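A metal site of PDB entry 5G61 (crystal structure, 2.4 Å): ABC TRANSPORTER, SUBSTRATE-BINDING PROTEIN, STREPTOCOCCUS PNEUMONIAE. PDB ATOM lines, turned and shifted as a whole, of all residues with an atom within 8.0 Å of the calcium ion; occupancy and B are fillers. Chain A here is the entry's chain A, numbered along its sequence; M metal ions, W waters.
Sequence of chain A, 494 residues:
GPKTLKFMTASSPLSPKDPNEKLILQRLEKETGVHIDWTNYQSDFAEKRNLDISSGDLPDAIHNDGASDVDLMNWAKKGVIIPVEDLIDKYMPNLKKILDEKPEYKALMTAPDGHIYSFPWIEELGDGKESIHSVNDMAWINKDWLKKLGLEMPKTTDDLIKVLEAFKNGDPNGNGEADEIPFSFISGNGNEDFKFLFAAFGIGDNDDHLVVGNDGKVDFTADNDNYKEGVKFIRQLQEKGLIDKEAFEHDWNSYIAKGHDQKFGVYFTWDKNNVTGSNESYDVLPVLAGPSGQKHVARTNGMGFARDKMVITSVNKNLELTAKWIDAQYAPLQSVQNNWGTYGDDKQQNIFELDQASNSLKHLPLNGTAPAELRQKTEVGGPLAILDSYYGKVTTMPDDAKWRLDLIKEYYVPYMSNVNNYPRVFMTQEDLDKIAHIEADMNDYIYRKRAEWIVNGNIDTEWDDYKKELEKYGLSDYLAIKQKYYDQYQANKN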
ATOM      1  N   ILE A 203     -32.417  18.145 -11.528  1.00  0.00           N
ATOM      2  CA  ILE A 203     -32.104  17.084 -12.490  1.00  0.00           C
ATOM      3  C   ILE A 203     -33.177  15.983 -12.438  1.00  0.00           C
ATOM      4  O   ILE A 203     -33.904  15.774 -13.418  1.00  0.00           O
ATOM      5  CB  ILE A 203     -30.668  16.538 -12.271  1.00  0.00           C
ATOM      6  CG1 ILE A 203     -29.659  17.685 -12.330  1.00  0.00           C
ATOM      7  CG2 ILE A 203     -30.294  15.490 -13.349  1.00  0.00           C
ATOM      8  CD1 ILE A 203     -28.214  17.307 -11.946  1.00  0.00           C
ATOM      9  N   HIS A 209     -32.320   6.285 -16.258  1.00  0.00           N
ATOM     10  CA  HIS A 209     -31.318   6.930 -15.414  1.00  0.00           C
ATOM     11  C   HIS A 209     -30.347   7.755 -16.259  1.00  0.00           C
ATOM     12  O   HIS A 209     -29.162   7.832 -15.947  1.00  0.00           O
ATOM     13  CB  HIS A 209     -30.574   5.894 -14.572  1.00  0.00           C
ATOM     14  CG  HIS A 209     -31.490   4.950 -13.879  1.00  0.00           C
ATOM     15  ND1 HIS A 209     -32.539   5.388 -13.087  1.00  0.00           N
ATOM     16  CD2 HIS A 209     -31.541   3.602 -13.850  1.00  0.00           C
ATOM     17  CE1 HIS A 209     -33.174   4.341 -12.591  1.00  0.00           C
ATOM     18  NE2 HIS A 209     -32.588   3.244 -13.033  1.00  0.00           N
ATOM     19  N   LEU A 210     -30.871   8.355 -17.334  1.00  0.00           N
ATOM     20  CA  LEU A 210     -30.082   9.092 -18.315  1.00  0.00           C
ATOM     21  C   LEU A 210     -30.822  10.357 -18.752  1.00  0.00           C
ATOM     22  O   LEU A 210     -31.961  10.278 -19.235  1.00  0.00           O
ATOM     23  CB  LEU A 210     -29.797   8.236 -19.552  1.00  0.00           C
ATOM     24  CG  LEU A 210     -28.461   7.503 -19.623  1.00  0.00           C
ATOM     25  CD1 LEU A 210     -28.254   6.979 -21.038  1.00  0.00           C
ATOM     26  CD2 LEU A 210     -27.292   8.410 -19.209  1.00  0.00           C
ATOM     27  N   VAL A 211     -30.164  11.506 -18.608  1.00  0.00           N
ATOM     28  CA  VAL A 211     -30.612  12.755 -19.183  1.00  0.00           C
ATOM     29  C   VAL A 211     -29.441  13.398 -19.921  1.00  0.00           C
ATOM     30  O   VAL A 211     -28.275  12.987 -19.780  1.00  0.00           O
ATOM     31  CB  VAL A 211     -31.217  13.706 -18.134  1.00  0.00           C
ATOM     32  CG1 VAL A 211     -32.369  13.049 -17.413  1.00  0.00           C
ATOM     33  CG2 VAL A 211     -30.149  14.203 -17.142  1.00  0.00           C
ATOM     34  N   VAL A 218     -24.109  13.834 -21.519  1.00  0.00           N
ATOM     35  CA  VAL A 218     -25.129  12.961 -20.936  1.00  0.00           C
ATOM     36  C   VAL A 218     -24.813  12.742 -19.460  1.00  0.00           C
ATOM     37  O   VAL A 218     -23.640  12.621 -19.067  1.00  0.00           O
ATOM     38  CB  VAL A 218     -25.261  11.633 -21.681  1.00  0.00           C
ATOM     39  CG1 VAL A 218     -25.222  11.858 -23.186  1.00  0.00           C
ATOM     40  CG2 VAL A 218     -24.219  10.608 -21.237  1.00  0.00           C
ATOM     41  N   ASP A 219     -25.855  12.708 -18.631  1.00  0.00           N
ATOM     42  CA  ASP A 219     -25.691  12.505 -17.205  1.00  0.00           C
ATOM     43  C   ASP A 219     -26.385  11.210 -16.779  1.00  0.00           C
ATOM     44  O   ASP A 219     -27.583  11.062 -16.958  1.00  0.00           O
ATOM     45  CB  ASP A 219     -26.268  13.661 -16.384  1.00  0.00           C
ATOM     46  CG  ASP A 219     -25.967  13.472 -14.917  1.00  0.00           C
ATOM     47  OD1 ASP A 219     -25.138  12.598 -14.602  1.00  0.00           O
ATOM     48  OD2 ASP A 219     -26.498  14.170 -14.058  1.00  0.00           O
ATOM     49  N   PHE A 220     -25.617  10.326 -16.160  1.00  0.00           N
ATOM     50  CA  PHE A 220     -26.227   9.206 -15.435  1.00  0.00           C
ATOM     51  C   PHE A 220     -26.870   9.758 -14.164  1.00  0.00           C
ATOM     52  O   PHE A 220     -26.181  10.186 -13.238  1.00  0.00           O
ATOM     53  CB  PHE A 220     -25.190   8.128 -15.161  1.00  0.00           C
ATOM     54  CG  PHE A 220     -25.725   6.953 -14.389  1.00  0.00           C
ATOM     55  CD1 PHE A 220     -26.437   5.944 -15.028  1.00  0.00           C
ATOM     56  CD2 PHE A 220     -25.469   6.826 -13.026  1.00  0.00           C
ATOM     57  CE1 PHE A 220     -26.904   4.858 -14.323  1.00  0.00           C
ATOM     58  CE2 PHE A 220     -25.925   5.736 -12.306  1.00  0.00           C
ATOM     59  CZ  PHE A 220     -26.652   4.757 -12.952  1.00  0.00           C
ATOM     60  N   THR A 221     -28.200   9.762 -14.118  1.00  0.00           N
ATOM     61  CA  THR A 221     -28.882  10.501 -13.068  1.00  0.00           C
ATOM     62  C   THR A 221     -28.700   9.858 -11.706  1.00  0.00           C
ATOM     63  O   THR A 221     -28.679  10.570 -10.692  1.00  0.00           O
ATOM     64  CB  THR A 221     -30.370  10.611 -13.399  1.00  0.00           C
ATOM     65  OG1 THR A 221     -30.924   9.300 -13.601  1.00  0.00           O
ATOM     66  CG2 THR A 221     -30.558  11.407 -14.652  1.00  0.00           C
ATOM     67  N   ALA A 222     -28.556   8.525 -11.640  1.00  0.00           N
ATOM     68  CA  ALA A 222     -28.651   7.836 -10.350  1.00  0.00           C
ATOM     69  C   ALA A 222     -27.362   7.877  -9.521  1.00  0.00           C
ATOM     70  O   ALA A 222     -27.308   7.219  -8.469  1.00  0.00           O
ATOM     71  CB  ALA A 222     -29.124   6.387 -10.550  1.00  0.00           C
ATOM     72  N   ASP A 223     -26.337   8.621  -9.921  1.00  0.00           N
ATOM     73  CA  ASP A 223     -25.200   8.882  -9.052  1.00  0.00           C
ATOM     74  C   ASP A 223     -25.098  10.348  -8.631  1.00  0.00           C
ATOM     75  O   ASP A 223     -24.122  10.739  -7.970  1.00  0.00           O
ATOM     76  CB  ASP A 223     -23.901   8.358  -9.691  1.00  0.00           C
ATOM     77  CG  ASP A 223     -23.416   9.170 -10.912  1.00  0.00           C
ATOM     78  OD1 ASP A 223     -24.170   9.985 -11.492  1.00  0.00           O
ATOM     79  OD2 ASP A 223     -22.241   8.963 -11.299  1.00  0.00           O
ATOM     80  N   ASN A 224     -26.106  11.162  -8.929  1.00  0.00           N
ATOM     81  CA  ASN A 224     -26.036  12.569  -8.548  1.00  0.00           C
ATOM     82  C   ASN A 224     -26.367  12.767  -7.073  1.00  0.00           C
ATOM     83  O   ASN A 224     -27.087  11.990  -6.449  1.00  0.00           O
ATOM     84  CB  ASN A 224     -27.024  13.408  -9.367  1.00  0.00           C
ATOM     85  CG  ASN A 224     -26.765  13.320 -10.843  1.00  0.00           C
ATOM     86  OD1 ASN A 224     -25.651  13.008 -11.282  1.00  0.00           O
ATOM     87  ND2 ASN A 224     -27.797  13.585 -11.632  1.00  0.00           N
ATOM     88  N   ASP A 225     -25.857  13.881  -6.529  1.00  0.00           N
ATOM     89  CA  ASP A 225     -26.252  14.296  -5.189  1.00  0.00           C
ATOM     90  C   ASP A 225     -27.740  14.624  -5.127  1.00  0.00           C
ATOM     91  O   ASP A 225     -28.378  14.419  -4.086  1.00  0.00           O
ATOM     92  CB  ASP A 225     -25.420  15.503  -4.735  1.00  0.00           C
ATOM     93  CG  ASP A 225     -23.988  15.160  -4.447  1.00  0.00           C
ATOM     94  OD1 ASP A 225     -23.731  13.977  -4.133  1.00  0.00           O
ATOM     95  OD2 ASP A 225     -23.121  16.048  -4.506  1.00  0.00           O
ATOM     96  N   ASN A 226     -28.267  15.202  -6.205  1.00  0.00           N
ATOM     97  CA  ASN A 226     -29.698  15.451  -6.324  1.00  0.00           C
ATOM     98  C   ASN A 226     -30.469  14.152  -6.193  1.00  0.00           C
ATOM     99  O   ASN A 226     -31.554  14.107  -5.597  1.00  0.00           O
ATOM    100  CB  ASN A 226     -30.014  16.091  -7.666  1.00  0.00           C
ATOM    101  CG  ASN A 226     -29.131  17.291  -7.985  1.00  0.00           C
ATOM    102  OD1 ASN A 226     -27.961  17.139  -8.282  1.00  0.00           O
ATOM    103  ND2 ASN A 226     -29.693  18.485  -7.928  1.00  0.00           N
ATOM    104  N   TYR A 227     -29.923  13.083  -6.775  1.00  0.00           N
ATOM    105  CA  TYR A 227     -30.560  11.796  -6.675  1.00  0.00           C
ATOM    106  C   TYR A 227     -30.556  11.291  -5.232  1.00  0.00           C
ATOM    107  O   TYR A 227     -31.563  10.798  -4.744  1.00  0.00           O
ATOM    108  CB  TYR A 227     -29.855  10.802  -7.605  1.00  0.00           C
ATOM    109  CG  TYR A 227     -30.455   9.430  -7.599  1.00  0.00           C
ATOM    110  CD1 TYR A 227     -30.056   8.476  -6.667  1.00  0.00           C
ATOM    111  CD2 TYR A 227     -31.427   9.076  -8.531  1.00  0.00           C
ATOM    112  CE1 TYR A 227     -30.598   7.207  -6.681  1.00  0.00           C
ATOM    113  CE2 TYR A 227     -31.967   7.840  -8.553  1.00  0.00           C
ATOM    114  CZ  TYR A 227     -31.564   6.895  -7.622  1.00  0.00           C
ATOM    115  OH  TYR A 227     -32.141   5.629  -7.661  1.00  0.00           O
ATOM    116  N   LYS A 467     -21.394   4.287  -5.234  1.00  0.00           N
ATOM    117  CA  LYS A 467     -20.826   4.856  -6.452  1.00  0.00           C
ATOM    118  C   LYS A 467     -19.598   4.070  -6.918  1.00  0.00           C
ATOM    119  O   LYS A 467     -19.398   3.870  -8.125  1.00  0.00           O
ATOM    120  CB  LYS A 467     -20.503   6.333  -6.238  1.00  0.00           C
ATOM    121  CG  LYS A 467     -21.713   7.192  -5.883  1.00  0.00           C
ATOM    122  CD  LYS A 467     -21.465   8.694  -6.160  1.00  0.00           C
ATOM    123  CE  LYS A 467     -20.641   9.387  -5.040  1.00  0.00           C
ATOM    124  NZ  LYS A 467     -20.352  10.846  -5.304  1.00  0.00           N
ATOM    125  N   LEU A 475     -19.711   1.928 -15.039  1.00  0.00           N
ATOM    126  CA  LEU A 475     -20.483   3.130 -15.354  1.00  0.00           C
ATOM    127  C   LEU A 475     -19.719   4.023 -16.322  1.00  0.00           C
ATOM    128  O   LEU A 475     -20.270   4.453 -17.337  1.00  0.00           O
ATOM    129  CB  LEU A 475     -20.836   3.872 -14.065  1.00  0.00           C
ATOM    130  CG  LEU A 475     -21.722   5.110 -14.229  1.00  0.00           C
ATOM    131  CD1 LEU A 475     -22.983   4.744 -14.980  1.00  0.00           C
ATOM    132  CD2 LEU A 475     -22.026   5.724 -12.864  1.00  0.00           C
ATOM    133  N   LEU A 479     -21.162   5.107 -19.635  1.00  0.00           N
ATOM    134  CA  LEU A 479     -21.433   6.496 -19.947  1.00  0.00           C
ATOM    135  C   LEU A 479     -20.646   6.944 -21.159  1.00  0.00           C
ATOM    136  O   LEU A 479     -21.134   7.780 -21.938  1.00  0.00           O
ATOM    137  CB  LEU A 479     -21.110   7.339 -18.713  1.00  0.00           C
ATOM    138  CG  LEU A 479     -22.022   8.487 -18.289  1.00  0.00           C
ATOM    139  CD1 LEU A 479     -23.482   8.167 -18.489  1.00  0.00           C
ATOM    140  CD2 LEU A 479     -21.760   8.787 -16.808  1.00  0.00           C
HETATM  141 CA    CA M   1     -24.303  11.891 -12.848  1.00  0.00          CA
HETATM  142  O   HOH W   1     -23.174  14.152 -13.444  1.00  0.00           O
HETATM  143  O   HOH W   2     -22.221  12.448 -11.763  1.00  0.00           O
HETATM  144  O   HOH W   3     -23.089  10.926 -14.663  1.00  0.00           O
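Of the 17 residues printed, 4 come within 4 Å of the calcium ion.
The calcium ion is bound by OD1 of Asp 219 (2.1 Å), OD1 of Asp 223 (2.3 Å), OD1 of Asn 224 (2.3 Å), water W3 (2.4 Å), water W2 (2.4 Å), O of Phe 220 (2.6 Å) and water W1 (2.6 Å).
O of Val 211 sits at hydrogen-bond distance from N of Asp 219, 2.7 Å away.
The side-chain amide nitrogen (ND2) of Asn 224 lies within hydrogen-bond range of the backbone carbonyl oxygen (O) of Thr 221, 3.3 Å away.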
